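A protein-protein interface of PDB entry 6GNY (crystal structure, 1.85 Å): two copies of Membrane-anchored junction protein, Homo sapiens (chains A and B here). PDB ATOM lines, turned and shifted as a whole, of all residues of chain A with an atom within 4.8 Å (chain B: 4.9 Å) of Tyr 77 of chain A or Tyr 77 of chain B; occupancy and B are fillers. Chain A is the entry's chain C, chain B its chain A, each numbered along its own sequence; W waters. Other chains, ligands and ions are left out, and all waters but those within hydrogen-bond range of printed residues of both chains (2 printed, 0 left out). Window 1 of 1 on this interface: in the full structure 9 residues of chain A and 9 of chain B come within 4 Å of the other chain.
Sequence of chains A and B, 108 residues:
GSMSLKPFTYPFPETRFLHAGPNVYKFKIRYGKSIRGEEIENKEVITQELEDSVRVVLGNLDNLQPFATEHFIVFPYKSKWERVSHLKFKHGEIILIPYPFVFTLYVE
Water W1 lies within hydrogen-bond range of the backbone carbonyl oxygen of Leu 64 of chain B (2.6 Å) and the backbone carbonyl oxygen of Lys 78 of chain A (2.8 Å). Water W2 lies within hydrogen-bond range of O of Leu 64 of chain A (2.7 Å), O of Lys 78 of chain B (2.9 Å) and NE2 of Gln 65 of chain A (3.5 Å).
The side-chain amide nitrogen (NE2) of Gln 65 of chain B lies within hydrogen-bond range of the backbone carbonyl oxygen (O) of Lys 78 of chain A, at 3.3 Å. The backbone carbonyl oxygen of Pro 76 of chain B is in hydrogen-bond range of the side-chain hydroxyl of Tyr 77 of chain A, at 2.8 Å. The side-chain hydroxyl of Tyr 77 of chain B is in hydrogen-bond range of the backbone carbonyl oxygen of Pro 76 of chain A. The side-chain amide nitrogen (NE2) of Gln 65 of chain A is in hydrogen-bond range of the backbone carbonyl oxygen (O) of Lys 78 of chain B, at 3.1 Å.
Tyr 77 of chain B touches Leu 64 of chain A. Gln 65 of chain A touches Tyr 77 of chain B. Ser 79 of chain B touches Gln 65 of chain A. Tyr 77 of chain B touches Pro 66 of chain A (CZ to CD, 3.8 Å). Pro 66 of chain A touches Tyr 106 of chain B (CG to CE1, 3.9 Å). Tyr 77 of chain B touches Phe 75 of chain A (OH to C, 3.0 Å). Leu 64 of chain B touches Tyr 77 of chain A. Tyr 77 of chain A touches Gln 65 of chain B (CE1 to CA, 3.9 Å). Tyr 77 of chain A touches Phe 75 of chain B (OH to C, 3.2 Å). Tyr 77 of chain A touches Tyr 77 of chain B.
Of the printed residues of chain B, Pro 76 of chain A touches Tyr 77. Of the printed residues of chain A, Gln 65 of chain B touches Tyr 77 (3.9 Å), Lys 78 (3.3 Å) and Ser 79 (3.9 Å). Printed residues of chain A within 4 Å of Pro 76 of chain B: Tyr 77 (2.8 Å). Tyr 77 of chain B touches just these residues of chain A: Leu 64, Gln 65, Pro 66, Phe 75, Pro 76 and Tyr 77. Printed residues of chain A within 4 Å of Ser 79 of chain B: Gln 65. The nearest printed residue of chain A that does not touch Tyr 77 of chain B is Tyr 106 of chain A (6.2 Å). The nearest printed residue of chain A that does not touch Tyr 106 of chain B is Gln 65 of chain A (4.4 Å).
N of Phe 75 of chain B is in hydrogen-bond range of O of Tyr 106 of chain B. N of Thr 104 of chain B lies within hydrogen-bond range of O of Tyr 77 of chain B, at 2.7 Å. O of Ser 79 of chain B lies within hydrogen-bond range of N of Val 102 of chain B, at 2.7 Å. The backbone NH of Phe 75 of chain A lies within hydrogen-bond range of the backbone carbonyl oxygen of Tyr 106 of chain A. The backbone carbonyl oxygen of Tyr 77 of chain A lies within hydrogen-bond range of the backbone NH of Thr 104 of chain A (2.8 Å). N of Val 102 of chain A lies within hydrogen-bond range of O of Ser 79 of chain A, at 2.7 Å.
Gln 65 of chain A touches Tyr 77 of chain B, and with the chains exchanged Tyr 77 of chain A touches Gln 65 of chain B. Gln 65 of chain A touches Lys 78 of chain B, and with the chains exchanged Lys 78 of chain A touches Gln 65 of chain B. Phe 75 of chain B touches its own counterpart, Phe 75 of chain A. Phe 75 of chain A touches Tyr 77 of chain B, and with the chains exchanged Tyr 77 of chain A touches Phe 75 of chain B. Positions printed for both chains: 64, 65, 66, 75, 76, 77, 78, 79, 102, 103, 104 and 106. Of the 18 pairs that touch across the chains among the printed residues, 18 have their exchanged pair printed and touching as well.
Hydrophobic or aromatic side chains of chain A that line the printed part of chain B: Pro 66, Phe 75, Pro 76, Tyr 77 and Tyr 106. Among the printed residues, 18 pairs touch across the chains. Among the printed residues, no Asp or Glu carboxylate lies within 4 Å of a Lys or Arg side-chain nitrogen of the other chain.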
ATOM      1  N   LEU A  64       8.174  -0.409 -29.655  1.00  0.00           N
ATOM      2  CA  LEU A  64       8.321   1.010 -29.940  1.00  0.00           C
ATOM      3  C   LEU A  64       8.497   1.791 -28.644  1.00  0.00           C
ATOM      4  O   LEU A  64       7.824   1.532 -27.643  1.00  0.00           O
ATOM      5  CB  LEU A  64       7.105   1.527 -30.711  1.00  0.00           C
ATOM      6  CG  LEU A  64       6.876   0.982 -32.126  1.00  0.00           C
ATOM      7  CD1 LEU A  64       5.686   1.682 -32.752  1.00  0.00           C
ATOM      8  CD2 LEU A  64       8.103   1.140 -33.015  1.00  0.00           C
ATOM      9  N   GLN A  65       9.423   2.745 -28.666  1.00  0.00           N
ATOM     10  CA  GLN A  65       9.706   3.609 -27.532  1.00  0.00           C
ATOM     11  C   GLN A  65      10.100   4.967 -28.089  1.00  0.00           C
ATOM     12  O   GLN A  65      10.629   5.042 -29.206  1.00  0.00           O
ATOM     13  CB  GLN A  65      10.831   3.049 -26.647  1.00  0.00           C
ATOM     14  CG  GLN A  65      10.559   1.655 -26.079  1.00  0.00           C
ATOM     15  CD  GLN A  65       9.399   1.632 -25.097  1.00  0.00           C
ATOM     16  OE1 GLN A  65       9.061   2.650 -24.495  1.00  0.00           O
ATOM     17  NE2 GLN A  65       8.780   0.465 -24.937  1.00  0.00           N
ATOM     18  N   PRO A  66       9.845   6.050 -27.363  1.00  0.00           N
ATOM     19  CA  PRO A  66      10.279   7.365 -27.841  1.00  0.00           C
ATOM     20  C   PRO A  66      11.790   7.506 -27.746  1.00  0.00           C
ATOM     21  O   PRO A  66      12.461   6.817 -26.977  1.00  0.00           O
ATOM     22  CB  PRO A  66       9.562   8.343 -26.905  1.00  0.00           C
ATOM     23  CG  PRO A  66       9.371   7.576 -25.652  1.00  0.00           C
ATOM     24  CD  PRO A  66       9.220   6.127 -26.031  1.00  0.00           C
ATOM     25  N   PHE A  75       8.057  10.260 -31.069  1.00  0.00           N
ATOM     26  CA  PHE A  75       7.128   9.357 -30.394  1.00  0.00           C
ATOM     27  C   PHE A  75       6.485   8.439 -31.429  1.00  0.00           C
ATOM     28  O   PHE A  75       5.473   8.805 -32.044  1.00  0.00           O
ATOM     29  CB  PHE A  75       6.051  10.150 -29.649  1.00  0.00           C
ATOM     30  CG  PHE A  75       6.586  11.044 -28.560  1.00  0.00           C
ATOM     31  CD1 PHE A  75       6.686  10.585 -27.259  1.00  0.00           C
ATOM     32  CD2 PHE A  75       6.970  12.347 -28.837  1.00  0.00           C
ATOM     33  CE1 PHE A  75       7.163  11.405 -26.251  1.00  0.00           C
ATOM     34  CE2 PHE A  75       7.451  13.171 -27.838  1.00  0.00           C
ATOM     35  CZ  PHE A  75       7.548  12.699 -26.541  1.00  0.00           C
ATOM     36  N   PRO A  76       7.017   7.238 -31.657  1.00  0.00           N
ATOM     37  CA  PRO A  76       6.421   6.351 -32.664  1.00  0.00           C
ATOM     38  C   PRO A  76       5.252   5.549 -32.109  1.00  0.00           C
ATOM     39  O   PRO A  76       5.246   5.133 -30.946  1.00  0.00           O
ATOM     40  CB  PRO A  76       7.589   5.440 -33.059  1.00  0.00           C
ATOM     41  CG  PRO A  76       8.412   5.354 -31.809  1.00  0.00           C
ATOM     42  CD  PRO A  76       8.285   6.697 -31.130  1.00  0.00           C
ATOM     43  N   TYR A  77       4.252   5.340 -32.966  1.00  0.00           N
ATOM     44  CA  TYR A  77       3.056   4.579 -32.632  1.00  0.00           C
ATOM     45  C   TYR A  77       2.647   3.713 -33.814  1.00  0.00           C
ATOM     46  O   TYR A  77       2.860   4.082 -34.970  1.00  0.00           O
ATOM     47  CB  TYR A  77       1.889   5.492 -32.258  1.00  0.00           C
ATOM     48  CG  TYR A  77       1.967   6.006 -30.846  1.00  0.00           C
ATOM     49  CD1 TYR A  77       1.319   5.347 -29.816  1.00  0.00           C
ATOM     50  CD2 TYR A  77       2.709   7.136 -30.539  1.00  0.00           C
ATOM     51  CE1 TYR A  77       1.389   5.809 -28.516  1.00  0.00           C
ATOM     52  CE2 TYR A  77       2.786   7.609 -29.241  1.00  0.00           C
ATOM     53  CZ  TYR A  77       2.129   6.937 -28.235  1.00  0.00           C
ATOM     54  OH  TYR A  77       2.207   7.398 -26.937  1.00  0.00           O
ATOM     55  N   LYS A  78       2.052   2.561 -33.511  1.00  0.00           N
ATOM     56  CA  LYS A  78       1.428   1.702 -34.507  1.00  0.00           C
ATOM     57  C   LYS A  78      -0.085   1.752 -34.356  1.00  0.00           C
ATOM     58  O   LYS A  78      -0.609   1.909 -33.250  1.00  0.00           O
ATOM     59  CB  LYS A  78       1.860   0.238 -34.374  1.00  0.00           C
ATOM     60  CG  LYS A  78       3.334   0.006 -34.280  1.00  0.00           C
ATOM     61  CD  LYS A  78       3.687  -1.441 -34.599  1.00  0.00           C
ATOM     62  CE  LYS A  78       3.084  -2.402 -33.598  1.00  0.00           C
ATOM     63  NZ  LYS A  78       3.615  -3.778 -33.783  1.00  0.00           N
ATOM     64  N   SER A  79      -0.781   1.611 -35.481  1.00  0.00           N
ATOM     65  CA  SER A  79      -2.227   1.454 -35.494  1.00  0.00           C
ATOM     66  C   SER A  79      -2.584   0.456 -36.585  1.00  0.00           C
ATOM     67  O   SER A  79      -1.830   0.257 -37.540  1.00  0.00           O
ATOM     68  CB  SER A  79      -2.945   2.792 -35.728  1.00  0.00           C
ATOM     69  OG  SER A  79      -2.531   3.386 -36.951  1.00  0.00           O
ATOM     70  N   VAL A 102       0.110   0.492 -39.431  1.00  0.00           N
ATOM     71  CA  VAL A 102       0.609   1.780 -39.902  1.00  0.00           C
ATOM     72  C   VAL A 102       1.443   2.408 -38.794  1.00  0.00           C
ATOM     73  O   VAL A 102       1.028   2.425 -37.630  1.00  0.00           O
ATOM     74  CB  VAL A 102      -0.555   2.704 -40.298  1.00  0.00           C
ATOM     75  CG1 VAL A 102      -0.024   4.028 -40.827  1.00  0.00           C
ATOM     76  CG2 VAL A 102      -1.454   2.019 -41.318  1.00  0.00           C
ATOM     77  N   PHE A 103       2.615   2.932 -39.152  1.00  0.00           N
ATOM     78  CA  PHE A 103       3.503   3.593 -38.201  1.00  0.00           C
ATOM     79  C   PHE A 103       3.327   5.101 -38.320  1.00  0.00           C
ATOM     80  O   PHE A 103       3.457   5.659 -39.415  1.00  0.00           O
ATOM     81  CB  PHE A 103       4.965   3.219 -38.446  1.00  0.00           C
ATOM     82  CG  PHE A 103       5.276   1.782 -38.169  1.00  0.00           C
ATOM     83  CD1 PHE A 103       5.352   0.868 -39.204  1.00  0.00           C
ATOM     84  CD2 PHE A 103       5.493   1.343 -36.874  1.00  0.00           C
ATOM     85  CE1 PHE A 103       5.633  -0.459 -38.954  1.00  0.00           C
ATOM     86  CE2 PHE A 103       5.779   0.019 -36.620  1.00  0.00           C
ATOM     87  CZ  PHE A 103       5.848  -0.882 -37.663  1.00  0.00           C
ATOM     88  N   THR A 104       3.004   5.753 -37.209  1.00  0.00           N
ATOM     89  CA  THR A 104       2.951   7.207 -37.147  1.00  0.00           C
ATOM     90  C   THR A 104       4.085   7.687 -36.252  1.00  0.00           C
ATOM     91  O   THR A 104       4.187   7.269 -35.090  1.00  0.00           O
ATOM     92  CB  THR A 104       1.605   7.700 -36.619  1.00  0.00           C
ATOM     93  OG1 THR A 104       0.547   7.197 -37.440  1.00  0.00           O
ATOM     94  CG2 THR A 104       1.559   9.231 -36.619  1.00  0.00           C
ATOM     95  N   TYR A 106       5.254  10.826 -34.420  1.00  0.00           N
ATOM     96  CA  TYR A 106       4.948  12.177 -33.956  1.00  0.00           C
ATOM     97  C   TYR A 106       6.280  12.835 -33.625  1.00  0.00           C
ATOM     98  O   TYR A 106       6.896  12.534 -32.602  1.00  0.00           O
ATOM     99  CB  TYR A 106       4.010  12.146 -32.754  1.00  0.00           C
ATOM    100  CG  TYR A 106       2.665  11.523 -33.058  1.00  0.00           C
ATOM    101  CD1 TYR A 106       2.428  10.183 -32.793  1.00  0.00           C
ATOM    102  CD2 TYR A 106       1.634  12.274 -33.607  1.00  0.00           C
ATOM    103  CE1 TYR A 106       1.203   9.605 -33.064  1.00  0.00           C
ATOM    104  CE2 TYR A 106       0.404  11.702 -33.888  1.00  0.00           C
ATOM    105  CZ  TYR A 106       0.195  10.367 -33.613  1.00  0.00           C
ATOM    106  OH  TYR A 106      -1.025   9.790 -33.882  1.00  0.00           O
ATOM    107  N   LEU B  64      -2.830   1.743 -27.617  1.00  0.00           N
ATOM    108  CA  LEU B  64      -2.344   2.968 -27.004  1.00  0.00           C
ATOM    109  C   LEU B  64      -2.150   4.047 -28.059  1.00  0.00           C
ATOM    110  O   LEU B  64      -1.638   3.791 -29.153  1.00  0.00           O
ATOM    111  CB  LEU B  64      -1.027   2.707 -26.276  1.00  0.00           C
ATOM    112  CG  LEU B  64      -1.097   1.772 -25.065  1.00  0.00           C
ATOM    113  CD1 LEU B  64       0.267   1.685 -24.405  1.00  0.00           C
ATOM    114  CD2 LEU B  64      -2.148   2.246 -24.071  1.00  0.00           C
ATOM    115  N   GLN B  65      -2.569   5.261 -27.722  1.00  0.00           N
ATOM    116  CA  GLN B  65      -2.449   6.407 -28.609  1.00  0.00           C
ATOM    117  C   GLN B  65      -2.235   7.642 -27.751  1.00  0.00           C
ATOM    118  O   GLN B  65      -2.732   7.699 -26.619  1.00  0.00           O
ATOM    119  CB  GLN B  65      -3.702   6.582 -29.485  1.00  0.00           C
ATOM    120  CG  GLN B  65      -4.030   5.384 -30.390  1.00  0.00           C
ATOM    121  CD  GLN B  65      -2.992   5.155 -31.485  1.00  0.00           C
ATOM    122  OE1 GLN B  65      -2.274   6.071 -31.878  1.00  0.00           O
ATOM    123  NE2 GLN B  65      -2.909   3.922 -31.975  1.00  0.00           N
ATOM    124  N   PRO B  66      -1.515   8.642 -28.253  1.00  0.00           N
ATOM    125  CA  PRO B  66      -1.362   9.881 -27.489  1.00  0.00           C
ATOM    126  C   PRO B  66      -2.658  10.673 -27.469  1.00  0.00           C
ATOM    127  O   PRO B  66      -3.496  10.563 -28.367  1.00  0.00           O
ATOM    128  CB  PRO B  66      -0.257  10.629 -28.243  1.00  0.00           C
ATOM    129  CG  PRO B  66      -0.356  10.136 -29.641  1.00  0.00           C
ATOM    130  CD  PRO B  66      -0.859   8.715 -29.571  1.00  0.00           C
ATOM    131  N   PHE B  75       1.749  10.810 -23.806  1.00  0.00           N
ATOM    132  CA  PHE B  75       2.229   9.797 -24.742  1.00  0.00           C
ATOM    133  C   PHE B  75       2.380   8.489 -23.981  1.00  0.00           C
ATOM    134  O   PHE B  75       3.411   8.274 -23.321  1.00  0.00           O
ATOM    135  CB  PHE B  75       3.568  10.206 -25.363  1.00  0.00           C
ATOM    136  CG  PHE B  75       3.509  11.472 -26.162  1.00  0.00           C
ATOM    137  CD1 PHE B  75       3.714  12.699 -25.553  1.00  0.00           C
ATOM    138  CD2 PHE B  75       3.275  11.435 -27.525  1.00  0.00           C
ATOM    139  CE1 PHE B  75       3.671  13.865 -26.287  1.00  0.00           C
ATOM    140  CE2 PHE B  75       3.231  12.597 -28.264  1.00  0.00           C
ATOM    141  CZ  PHE B  75       3.427  13.814 -27.648  1.00  0.00           C
ATOM    142  N   PRO B  76       1.388   7.600 -24.001  1.00  0.00           N
ATOM    143  CA  PRO B  76       1.519   6.350 -23.244  1.00  0.00           C
ATOM    144  C   PRO B  76       2.295   5.299 -24.024  1.00  0.00           C
ATOM    145  O   PRO B  76       2.167   5.176 -25.245  1.00  0.00           O
ATOM    146  CB  PRO B  76       0.064   5.920 -23.021  1.00  0.00           C
ATOM    147  CG  PRO B  76      -0.655   6.454 -24.225  1.00  0.00           C
ATOM    148  CD  PRO B  76       0.038   7.755 -24.580  1.00  0.00           C
ATOM    149  N   TYR B  77       3.106   4.535 -23.293  1.00  0.00           N
ATOM    150  CA  TYR B  77       3.915   3.469 -23.861  1.00  0.00           C
ATOM    151  C   TYR B  77       3.904   2.279 -22.919  1.00  0.00           C
ATOM    152  O   TYR B  77       3.866   2.439 -21.696  1.00  0.00           O
ATOM    153  CB  TYR B  77       5.361   3.926 -24.099  1.00  0.00           C
ATOM    154  CG  TYR B  77       5.535   4.729 -25.370  1.00  0.00           C
ATOM    155  CD1 TYR B  77       5.936   4.119 -26.548  1.00  0.00           C
ATOM    156  CD2 TYR B  77       5.289   6.093 -25.392  1.00  0.00           C
ATOM    157  CE1 TYR B  77       6.094   4.846 -27.713  1.00  0.00           C
ATOM    158  CE2 TYR B  77       5.437   6.827 -26.553  1.00  0.00           C
ATOM    159  CZ  TYR B  77       5.843   6.200 -27.707  1.00  0.00           C
ATOM    160  OH  TYR B  77       5.986   6.928 -28.866  1.00  0.00           O
ATOM    161  N   LYS B  78       3.956   1.081 -23.494  1.00  0.00           N
ATOM    162  CA  LYS B  78       4.127  -0.126 -22.701  1.00  0.00           C
ATOM    163  C   LYS B  78       5.499  -0.740 -22.954  1.00  0.00           C
ATOM    164  O   LYS B  78       6.057  -0.646 -24.053  1.00  0.00           O
ATOM    165  CB  LYS B  78       3.023  -1.152 -22.982  1.00  0.00           C
ATOM    166  CG  LYS B  78       2.884  -1.598 -24.417  1.00  0.00           C
ATOM    167  CD  LYS B  78       1.918  -2.780 -24.537  1.00  0.00           C
ATOM    168  CE  LYS B  78       0.585  -2.517 -23.839  1.00  0.00           C
ATOM    169  NZ  LYS B  78      -0.428  -3.575 -24.125  1.00  0.00           N
ATOM    170  N   SER B  79       6.036  -1.352 -21.904  1.00  0.00           N
ATOM    171  CA  SER B  79       7.274  -2.113 -21.956  1.00  0.00           C
ATOM    172  C   SER B  79       7.111  -3.328 -21.056  1.00  0.00           C
ATOM    173  O   SER B  79       6.232  -3.365 -20.194  1.00  0.00           O
ATOM    174  CB  SER B  79       8.478  -1.275 -21.513  1.00  0.00           C
ATOM    175  OG  SER B  79       8.290  -0.788 -20.197  1.00  0.00           O
ATOM    176  N   VAL B 102       4.639  -2.876 -18.125  1.00  0.00           N
ATOM    177  CA  VAL B 102       4.640  -1.578 -17.472  1.00  0.00           C
ATOM    178  C   VAL B 102       4.060  -0.552 -18.430  1.00  0.00           C
ATOM    179  O   VAL B 102       4.359  -0.564 -19.630  1.00  0.00           O
ATOM    180  CB  VAL B 102       6.069  -1.188 -17.056  1.00  0.00           C
ATOM    181  CG1 VAL B 102       6.094   0.226 -16.473  1.00  0.00           C
ATOM    182  CG2 VAL B 102       6.634  -2.204 -16.079  1.00  0.00           C
ATOM    183  N   PHE B 103       3.225   0.341 -17.911  1.00  0.00           N
ATOM    184  CA  PHE B 103       2.739   1.477 -18.685  1.00  0.00           C
ATOM    185  C   PHE B 103       3.445   2.738 -18.215  1.00  0.00           C
ATOM    186  O   PHE B 103       3.391   3.083 -17.030  1.00  0.00           O
ATOM    187  CB  PHE B 103       1.225   1.624 -18.552  1.00  0.00           C
ATOM    188  CG  PHE B 103       0.462   0.523 -19.212  1.00  0.00           C
ATOM    189  CD1 PHE B 103       0.239   0.547 -20.579  1.00  0.00           C
ATOM    190  CD2 PHE B 103      -0.008  -0.550 -18.481  1.00  0.00           C
ATOM    191  CE1 PHE B 103      -0.454  -0.470 -21.200  1.00  0.00           C
ATOM    192  CE2 PHE B 103      -0.704  -1.570 -19.097  1.00  0.00           C
ATOM    193  CZ  PHE B 103      -0.924  -1.530 -20.461  1.00  0.00           C
ATOM    194  N   THR B 104       4.100   3.423 -19.143  1.00  0.00           N
ATOM    195  CA  THR B 104       4.744   4.696 -18.857  1.00  0.00           C
ATOM    196  C   THR B 104       3.956   5.797 -19.546  1.00  0.00           C
ATOM    197  O   THR B 104       3.706   5.731 -20.754  1.00  0.00           O
ATOM    198  CB  THR B 104       6.200   4.716 -19.326  1.00  0.00           C
ATOM    199  OG1 THR B 104       6.927   3.653 -18.702  1.00  0.00           O
ATOM    200  CG2 THR B 104       6.856   6.047 -18.976  1.00  0.00           C
ATOM    201  N   TYR B 106       4.302   9.402 -20.616  1.00  0.00           N
ATOM    202  CA  TYR B 106       5.189  10.543 -20.842  1.00  0.00           C
ATOM    203  C   TYR B 106       4.319  11.785 -20.944  1.00  0.00           C
ATOM    204  O   TYR B 106       3.631  12.002 -21.946  1.00  0.00           O
ATOM    205  CB  TYR B 106       6.037  10.334 -22.091  1.00  0.00           C
ATOM    206  CG  TYR B 106       6.995   9.172 -21.985  1.00  0.00           C
ATOM    207  CD1 TYR B 106       6.635   7.909 -22.427  1.00  0.00           C
ATOM    208  CD2 TYR B 106       8.255   9.336 -21.423  1.00  0.00           C
ATOM    209  CE1 TYR B 106       7.507   6.843 -22.332  1.00  0.00           C
ATOM    210  CE2 TYR B 106       9.135   8.274 -21.324  1.00  0.00           C
ATOM    211  CZ  TYR B 106       8.753   7.029 -21.778  1.00  0.00           C
ATOM    212  OH  TYR B 106       9.620   5.967 -21.680  1.00  0.00           O
HETATM  213  O   HOH W   1      -0.651   1.717 -30.429  1.00  0.00           O
HETATM  214  O   HOH W   2       6.052  -0.304 -26.924  1.00  0.00           O
